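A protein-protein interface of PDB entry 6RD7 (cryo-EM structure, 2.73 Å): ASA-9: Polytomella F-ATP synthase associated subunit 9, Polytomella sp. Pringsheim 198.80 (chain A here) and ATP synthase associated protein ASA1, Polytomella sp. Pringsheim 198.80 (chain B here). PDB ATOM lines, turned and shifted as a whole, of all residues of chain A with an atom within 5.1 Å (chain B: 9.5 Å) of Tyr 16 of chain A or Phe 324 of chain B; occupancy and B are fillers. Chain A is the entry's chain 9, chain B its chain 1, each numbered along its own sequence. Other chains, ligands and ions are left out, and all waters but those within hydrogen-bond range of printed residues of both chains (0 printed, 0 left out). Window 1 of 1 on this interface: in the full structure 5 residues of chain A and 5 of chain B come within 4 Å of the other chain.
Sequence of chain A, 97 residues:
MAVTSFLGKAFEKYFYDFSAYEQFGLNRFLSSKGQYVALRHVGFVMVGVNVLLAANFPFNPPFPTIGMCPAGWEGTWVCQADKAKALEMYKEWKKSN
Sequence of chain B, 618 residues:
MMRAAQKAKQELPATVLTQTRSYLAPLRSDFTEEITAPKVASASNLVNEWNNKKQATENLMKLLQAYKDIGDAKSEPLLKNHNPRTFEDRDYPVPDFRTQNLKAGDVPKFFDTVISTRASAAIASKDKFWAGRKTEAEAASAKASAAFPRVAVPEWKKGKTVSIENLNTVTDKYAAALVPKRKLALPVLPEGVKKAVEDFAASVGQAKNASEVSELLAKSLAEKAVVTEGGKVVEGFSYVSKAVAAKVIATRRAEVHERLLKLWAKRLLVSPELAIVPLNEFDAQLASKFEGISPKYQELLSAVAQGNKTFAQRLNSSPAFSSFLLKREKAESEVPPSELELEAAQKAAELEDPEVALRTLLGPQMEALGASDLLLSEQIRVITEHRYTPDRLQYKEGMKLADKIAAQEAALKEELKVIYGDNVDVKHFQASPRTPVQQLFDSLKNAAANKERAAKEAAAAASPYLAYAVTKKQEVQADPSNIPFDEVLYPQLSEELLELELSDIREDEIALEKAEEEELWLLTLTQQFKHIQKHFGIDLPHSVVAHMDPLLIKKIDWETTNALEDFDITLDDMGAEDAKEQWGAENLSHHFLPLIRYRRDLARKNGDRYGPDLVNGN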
ATOM      1  N   GLY A   8     -15.907  21.299  11.162  1.00  0.00           N
ATOM      2  CA  GLY A   8     -14.775  20.968  10.316  1.00  0.00           C
ATOM      3  C   GLY A   8     -14.432  19.492  10.333  1.00  0.00           C
ATOM      4  O   GLY A   8     -14.186  18.897   9.284  1.00  0.00           O
ATOM      5  N   PHE A  11     -17.306  17.534   8.557  1.00  0.00           N
ATOM      6  CA  PHE A  11     -17.226  17.705   7.112  1.00  0.00           C
ATOM      7  C   PHE A  11     -16.007  17.000   6.540  1.00  0.00           C
ATOM      8  O   PHE A  11     -16.046  16.518   5.407  1.00  0.00           O
ATOM      9  CB  PHE A  11     -17.199  19.188   6.750  1.00  0.00           C
ATOM     10  CG  PHE A  11     -17.073  19.438   5.279  1.00  0.00           C
ATOM     11  CD1 PHE A  11     -18.063  19.017   4.409  1.00  0.00           C
ATOM     12  CD2 PHE A  11     -15.956  20.068   4.763  1.00  0.00           C
ATOM     13  CE1 PHE A  11     -17.950  19.233   3.052  1.00  0.00           C
ATOM     14  CE2 PHE A  11     -15.838  20.287   3.406  1.00  0.00           C
ATOM     15  CZ  PHE A  11     -16.836  19.868   2.552  1.00  0.00           C
ATOM     16  N   GLU A  12     -14.925  16.899   7.317  1.00  0.00           N
ATOM     17  CA  GLU A  12     -13.746  16.177   6.855  1.00  0.00           C
ATOM     18  C   GLU A  12     -14.021  14.686   6.729  1.00  0.00           C
ATOM     19  O   GLU A  12     -13.664  14.062   5.719  1.00  0.00           O
ATOM     20  CB  GLU A  12     -12.578  16.431   7.804  1.00  0.00           C
ATOM     21  CG  GLU A  12     -11.469  15.403   7.732  1.00  0.00           C
ATOM     22  CD  GLU A  12     -10.540  15.470   8.920  1.00  0.00           C
ATOM     23  OE1 GLU A  12      -9.700  14.560   9.072  1.00  0.00           O
ATOM     24  OE2 GLU A  12     -10.648  16.436   9.703  1.00  0.00           O
ATOM     25  N   LYS A  13     -14.682  14.097   7.728  1.00  0.00           N
ATOM     26  CA  LYS A  13     -14.951  12.665   7.654  1.00  0.00           C
ATOM     27  C   LYS A  13     -16.082  12.360   6.676  1.00  0.00           C
ATOM     28  O   LYS A  13     -16.187  11.239   6.167  1.00  0.00           O
ATOM     29  CB  LYS A  13     -15.239  12.094   9.045  1.00  0.00           C
ATOM     30  CG  LYS A  13     -16.500  12.570   9.733  1.00  0.00           C
ATOM     31  CD  LYS A  13     -16.600  11.911  11.107  1.00  0.00           C
ATOM     32  CE  LYS A  13     -17.868  12.301  11.851  1.00  0.00           C
ATOM     33  NZ  LYS A  13     -17.946  11.654  13.193  1.00  0.00           N
ATOM     34  N   TYR A  14     -16.929  13.351   6.377  1.00  0.00           N
ATOM     35  CA  TYR A  14     -17.883  13.176   5.283  1.00  0.00           C
ATOM     36  C   TYR A  14     -17.193  13.283   3.927  1.00  0.00           C
ATOM     37  O   TYR A  14     -17.533  12.558   2.987  1.00  0.00           O
ATOM     38  CB  TYR A  14     -19.010  14.205   5.389  1.00  0.00           C
ATOM     39  CG  TYR A  14     -19.760  14.425   4.093  1.00  0.00           C
ATOM     40  CD1 TYR A  14     -20.620  13.455   3.594  1.00  0.00           C
ATOM     41  CD2 TYR A  14     -19.608  15.602   3.368  1.00  0.00           C
ATOM     42  CE1 TYR A  14     -21.305  13.648   2.410  1.00  0.00           C
ATOM     43  CE2 TYR A  14     -20.288  15.802   2.181  1.00  0.00           C
ATOM     44  CZ  TYR A  14     -21.134  14.822   1.710  1.00  0.00           C
ATOM     45  OH  TYR A  14     -21.813  15.020   0.532  1.00  0.00           O
ATOM     46  N   PHE A  15     -16.220  14.186   3.812  1.00  0.00           N
ATOM     47  CA  PHE A  15     -15.585  14.465   2.533  1.00  0.00           C
ATOM     48  C   PHE A  15     -14.645  13.343   2.124  1.00  0.00           C
ATOM     49  O   PHE A  15     -14.568  12.985   0.945  1.00  0.00           O
ATOM     50  CB  PHE A  15     -14.837  15.795   2.633  1.00  0.00           C
ATOM     51  CG  PHE A  15     -14.261  16.285   1.337  1.00  0.00           C
ATOM     52  CD1 PHE A  15     -12.925  16.084   1.039  1.00  0.00           C
ATOM     53  CD2 PHE A  15     -15.045  16.978   0.436  1.00  0.00           C
ATOM     54  CE1 PHE A  15     -12.390  16.541  -0.143  1.00  0.00           C
ATOM     55  CE2 PHE A  15     -14.512  17.439  -0.749  1.00  0.00           C
ATOM     56  CZ  PHE A  15     -13.184  17.220  -1.036  1.00  0.00           C
ATOM     57  N   TYR A  16     -13.923  12.768   3.084  1.00  0.00           N
ATOM     58  CA  TYR A  16     -12.881  11.799   2.772  1.00  0.00           C
ATOM     59  C   TYR A  16     -13.340  10.358   2.953  1.00  0.00           C
ATOM     60  O   TYR A  16     -13.243   9.550   2.026  1.00  0.00           O
ATOM     61  CB  TYR A  16     -11.651  12.077   3.637  1.00  0.00           C
ATOM     62  CG  TYR A  16     -10.808  13.211   3.121  1.00  0.00           C
ATOM     63  CD1 TYR A  16     -10.748  14.417   3.798  1.00  0.00           C
ATOM     64  CD2 TYR A  16     -10.077  13.075   1.953  1.00  0.00           C
ATOM     65  CE1 TYR A  16      -9.982  15.453   3.329  1.00  0.00           C
ATOM     66  CE2 TYR A  16      -9.308  14.107   1.476  1.00  0.00           C
ATOM     67  CZ  TYR A  16      -9.264  15.292   2.168  1.00  0.00           C
ATOM     68  OH  TYR A  16      -8.497  16.322   1.696  1.00  0.00           O
ATOM     69  N   ASP A  17     -13.841  10.019   4.140  1.00  0.00           N
ATOM     70  CA  ASP A  17     -14.089   8.619   4.465  1.00  0.00           C
ATOM     71  C   ASP A  17     -15.427   8.150   3.910  1.00  0.00           C
ATOM     72  O   ASP A  17     -15.552   7.019   3.426  1.00  0.00           O
ATOM     73  CB  ASP A  17     -14.020   8.425   5.976  1.00  0.00           C
ATOM     74  CG  ASP A  17     -12.697   8.869   6.553  1.00  0.00           C
ATOM     75  OD1 ASP A  17     -12.686   9.833   7.346  1.00  0.00           O
ATOM     76  OD2 ASP A  17     -11.663   8.263   6.202  1.00  0.00           O
ATOM     77  N   PHE A  18     -16.445   9.003   3.984  1.00  0.00           N
ATOM     78  CA  PHE A  18     -17.737   8.671   3.401  1.00  0.00           C
ATOM     79  C   PHE A  18     -17.640   8.694   1.883  1.00  0.00           C
ATOM     80  O   PHE A  18     -17.235   9.695   1.286  1.00  0.00           O
ATOM     81  CB  PHE A  18     -18.807   9.652   3.885  1.00  0.00           C
ATOM     82  CG  PHE A  18     -20.213   9.265   3.508  1.00  0.00           C
ATOM     83  CD1 PHE A  18     -20.798   9.749   2.344  1.00  0.00           C
ATOM     84  CD2 PHE A  18     -20.958   8.434   4.327  1.00  0.00           C
ATOM     85  CE1 PHE A  18     -22.090   9.397   1.999  1.00  0.00           C
ATOM     86  CE2 PHE A  18     -22.253   8.081   3.989  1.00  0.00           C
ATOM     87  CZ  PHE A  18     -22.817   8.565   2.823  1.00  0.00           C
ATOM     88  N   PRO B 319       2.642  23.485   7.407  1.00  0.00           N
ATOM     89  CA  PRO B 319       1.213  23.831   7.512  1.00  0.00           C
ATOM     90  C   PRO B 319       0.385  23.470   6.292  1.00  0.00           C
ATOM     91  O   PRO B 319      -0.823  23.247   6.432  1.00  0.00           O
ATOM     92  CB  PRO B 319       1.233  25.349   7.723  1.00  0.00           C
ATOM     93  CG  PRO B 319       2.543  25.640   8.275  1.00  0.00           C
ATOM     94  CD  PRO B 319       3.492  24.656   7.694  1.00  0.00           C
ATOM     95  N   ALA B 320       0.996  23.379   5.111  1.00  0.00           N
ATOM     96  CA  ALA B 320       0.225  23.179   3.890  1.00  0.00           C
ATOM     97  C   ALA B 320      -0.302  21.755   3.785  1.00  0.00           C
ATOM     98  O   ALA B 320      -1.295  21.504   3.095  1.00  0.00           O
ATOM     99  CB  ALA B 320       1.076  23.534   2.677  1.00  0.00           C
ATOM    100  N   PHE B 321       0.345  20.807   4.457  1.00  0.00           N
ATOM    101  CA  PHE B 321      -0.210  19.466   4.548  1.00  0.00           C
ATOM    102  C   PHE B 321      -1.130  19.298   5.745  1.00  0.00           C
ATOM    103  O   PHE B 321      -1.613  18.189   5.987  1.00  0.00           O
ATOM    104  CB  PHE B 321       0.909  18.428   4.589  1.00  0.00           C
ATOM    105  CG  PHE B 321       1.398  18.028   3.234  1.00  0.00           C
ATOM    106  CD1 PHE B 321       0.762  17.034   2.519  1.00  0.00           C
ATOM    107  CD2 PHE B 321       2.483  18.662   2.664  1.00  0.00           C
ATOM    108  CE1 PHE B 321       1.208  16.676   1.265  1.00  0.00           C
ATOM    109  CE2 PHE B 321       2.933  18.309   1.415  1.00  0.00           C
ATOM    110  CZ  PHE B 321       2.295  17.317   0.714  1.00  0.00           C
ATOM    111  N   SER B 322      -1.372  20.365   6.499  1.00  0.00           N
ATOM    112  CA  SER B 322      -2.444  20.398   7.479  1.00  0.00           C
ATOM    113  C   SER B 322      -3.684  21.089   6.938  1.00  0.00           C
ATOM    114  O   SER B 322      -4.708  21.124   7.624  1.00  0.00           O
ATOM    115  CB  SER B 322      -1.977  21.099   8.754  1.00  0.00           C
ATOM    116  OG  SER B 322      -0.787  20.510   9.246  1.00  0.00           O
ATOM    117  N   SER B 323      -3.606  21.642   5.731  1.00  0.00           N
ATOM    118  CA  SER B 323      -4.760  22.209   5.062  1.00  0.00           C
ATOM    119  C   SER B 323      -5.691  21.094   4.611  1.00  0.00           C
ATOM    120  O   SER B 323      -5.284  19.940   4.474  1.00  0.00           O
ATOM    121  CB  SER B 323      -4.330  23.053   3.867  1.00  0.00           C
ATOM    122  OG  SER B 323      -3.564  22.278   2.966  1.00  0.00           O
ATOM    123  N   PHE B 324      -6.944  21.473   4.336  1.00  0.00           N
ATOM    124  CA  PHE B 324      -8.038  20.510   4.227  1.00  0.00           C
ATOM    125  C   PHE B 324      -7.883  19.593   3.021  1.00  0.00           C
ATOM    126  O   PHE B 324      -8.179  18.396   3.097  1.00  0.00           O
ATOM    127  CB  PHE B 324      -9.369  21.253   4.156  1.00  0.00           C
ATOM    128  CG  PHE B 324     -10.556  20.350   4.049  1.00  0.00           C
ATOM    129  CD1 PHE B 324     -11.027  19.685   5.162  1.00  0.00           C
ATOM    130  CD2 PHE B 324     -11.200  20.164   2.835  1.00  0.00           C
ATOM    131  CE1 PHE B 324     -12.111  18.853   5.071  1.00  0.00           C
ATOM    132  CE2 PHE B 324     -12.283  19.329   2.741  1.00  0.00           C
ATOM    133  CZ  PHE B 324     -12.740  18.672   3.860  1.00  0.00           C
ATOM    134  N   LEU B 325      -7.419  20.135   1.896  1.00  0.00           N
ATOM    135  CA  LEU B 325      -7.342  19.335   0.678  1.00  0.00           C
ATOM    136  C   LEU B 325      -6.155  18.385   0.714  1.00  0.00           C
ATOM    137  O   LEU B 325      -6.069  17.457  -0.096  1.00  0.00           O
ATOM    138  CB  LEU B 325      -7.264  20.251  -0.539  1.00  0.00           C
ATOM    139  CG  LEU B 325      -8.401  21.265  -0.642  1.00  0.00           C
ATOM    140  CD1 LEU B 325      -8.133  22.254  -1.753  1.00  0.00           C
ATOM    141  CD2 LEU B 325      -9.717  20.555  -0.866  1.00  0.00           C
ATOM    142  N   LEU B 326      -5.226  18.604   1.638  1.00  0.00           N
ATOM    143  CA  LEU B 326      -4.013  17.808   1.740  1.00  0.00           C
ATOM    144  C   LEU B 326      -3.838  17.157   3.105  1.00  0.00           C
ATOM    145  O   LEU B 326      -2.698  16.919   3.513  1.00  0.00           O
ATOM    146  CB  LEU B 326      -2.801  18.683   1.417  1.00  0.00           C
ATOM    147  CG  LEU B 326      -2.857  19.226  -0.008  1.00  0.00           C
ATOM    148  CD1 LEU B 326      -2.020  20.453  -0.192  1.00  0.00           C
ATOM    149  CD2 LEU B 326      -2.435  18.153  -0.961  1.00  0.00           C
ATOM    150  N   LYS B 327      -4.929  16.869   3.819  1.00  0.00           N
ATOM    151  CA  LYS B 327      -4.825  16.209   5.117  1.00  0.00           C
ATOM    152  C   LYS B 327      -4.379  14.763   4.965  1.00  0.00           C
ATOM    153  O   LYS B 327      -3.564  14.263   5.747  1.00  0.00           O
ATOM    154  CB  LYS B 327      -6.164  16.265   5.853  1.00  0.00           C
ATOM    155  CG  LYS B 327      -6.585  17.639   6.293  1.00  0.00           C
ATOM    156  CD  LYS B 327      -7.901  17.621   7.031  1.00  0.00           C
ATOM    157  CE  LYS B 327      -7.670  17.513   8.519  1.00  0.00           C
ATOM    158  NZ  LYS B 327      -6.984  18.721   9.046  1.00  0.00           N
ATOM    159  N   ARG B 328      -4.909  14.073   3.963  1.00  0.00           N
ATOM    160  CA  ARG B 328      -4.644  12.655   3.778  1.00  0.00           C
ATOM    161  C   ARG B 328      -3.535  12.383   2.777  1.00  0.00           C
ATOM    162  O   ARG B 328      -3.174  11.220   2.577  1.00  0.00           O
ATOM    163  CB  ARG B 328      -5.918  11.937   3.337  1.00  0.00           C
ATOM    164  CG  ARG B 328      -6.780  11.474   4.488  1.00  0.00           C
ATOM    165  CD  ARG B 328      -7.781  12.534   4.862  1.00  0.00           C
ATOM    166  NE  ARG B 328      -8.881  11.997   5.653  1.00  0.00           N
ATOM    167  CZ  ARG B 328      -9.079  12.277   6.933  1.00  0.00           C
ATOM    168  NH1 ARG B 328      -8.250  13.093   7.568  1.00  0.00           N
ATOM    169  NH2 ARG B 328     -10.108  11.748   7.576  1.00  0.00           N
ATOM    170  N   GLU B 329      -2.992  13.412   2.142  1.00  0.00           N
ATOM    171  CA  GLU B 329      -1.882  13.217   1.228  1.00  0.00           C
ATOM    172  C   GLU B 329      -0.572  13.167   1.996  1.00  0.00           C
ATOM    173  O   GLU B 329      -0.462  13.669   3.116  1.00  0.00           O
ATOM    174  CB  GLU B 329      -1.836  14.331   0.185  1.00  0.00           C
ATOM    175  CG  GLU B 329      -3.098  14.452  -0.640  1.00  0.00           C
ATOM    176  CD  GLU B 329      -3.452  13.169  -1.357  1.00  0.00           C
ATOM    177  OE1 GLU B 329      -4.623  12.742  -1.271  1.00  0.00           O
ATOM    178  OE2 GLU B 329      -2.564  12.586  -2.011  1.00  0.00           O
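The backbone carbonyl oxygen of Phe 324 of chain B sits at hydrogen-bond distance from the side-chain hydroxyl of Tyr 16 of chain A, at 2.5 Å.
The backbone carbonyl oxygen (O) of Leu 325 of chain B is in hydrogen-bond range of the side-chain hydroxyl (OH) of Tyr 16 of chain A (3.2 Å).
NH1 of Arg 328 of chain B is in salt-bridge range of OE1 of Glu 12 of chain A (2.6 Å).
The side-chain carboxylate of Asp 17 of chain A is in salt-bridge range of the guanidinium group of Arg 328 of chain B, 3.2 Å away.
Of the 11 printed residues of chain B, 5 touch a printed residue of chain A.
Printed residues of chain B that touch a printed residue of chain A: Phe 324, Leu 325, Leu 326, Lys 327 and Arg 328.
Hydrophobic or aromatic side chains of chain B within 4 Å of the printed part of chain A: Phe 324.
Along chain B the printed residues that touch a printed residue of chain A span positions 324 to 328.
Hydrophobic or aromatic side chains of chain A within 4 Å of the printed part of chain B: Phe 11, Phe 15 and Tyr 16.
Among the printed residues, 10 pairs touch across the chains.
Among the printed residues, Asp or Glu carboxylates within 4 Å of a Lys or Arg side-chain nitrogen of the other chain: Glu 12 of chain A with Arg 328 of chain B (2.6 Å) and Asp 17 of chain A with Arg 328 of chain B (3.2 Å).
Phe 11 of chain A touches Phe 324 of chain B.
CE1 of Phe 324 of chain B touches CA of Glu 12 of chain A (3.6 Å).
CE of Lys 327 of chain B touches OE2 of Glu 12 of chain A, 3.4 Å away.
Phe 324 of chain B touches Phe 15 of chain A.
OH of Tyr 16 of chain A touches N of Leu 326 of chain B (3.99 Å).
Arg 328 of chain B touches Tyr 16 of chain A (NE to CG, 3.4 Å).
Glu 12 of chain A touches three residues of chain B.
Tyr 14 of chain A touches none of the printed residues of chain B.
Of chain B, only Phe 324 (3.7 Å) comes within 4 Å of Phe 15 of chain A.
Of the printed residues of chain B, Tyr 16 of chain A touches Phe 324 (2.5 Å), Leu 325 (3.2 Å), Leu 326 (3.99 Å) and Arg 328 (3.4 Å).
Asp 17 of chain A touches just one residue of chain B: Arg 328.
Phe 321 of chain B touches none of the printed residues of chain A.
Of chain A, only Phe 11, Glu 12, Phe 15 and Tyr 16 come within 4 Å of Phe 324 of chain B.
Of the printed residues of chain A, Leu 326 of chain B touches Tyr 16.
Printed residues of chain A within 4 Å of Arg 328 of chain B: Glu 12 (2.6 Å), Tyr 16 (3.4 Å) and Asp 17 (3.2 Å).
The nearest residue of chain A that does not touch Phe 324 of chain B is Gly 8 of chain A (4.7 Å).
The nearest printed residue of chain A that does not touch Leu 325 of chain B is Phe 15 of chain A (4.8 Å).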
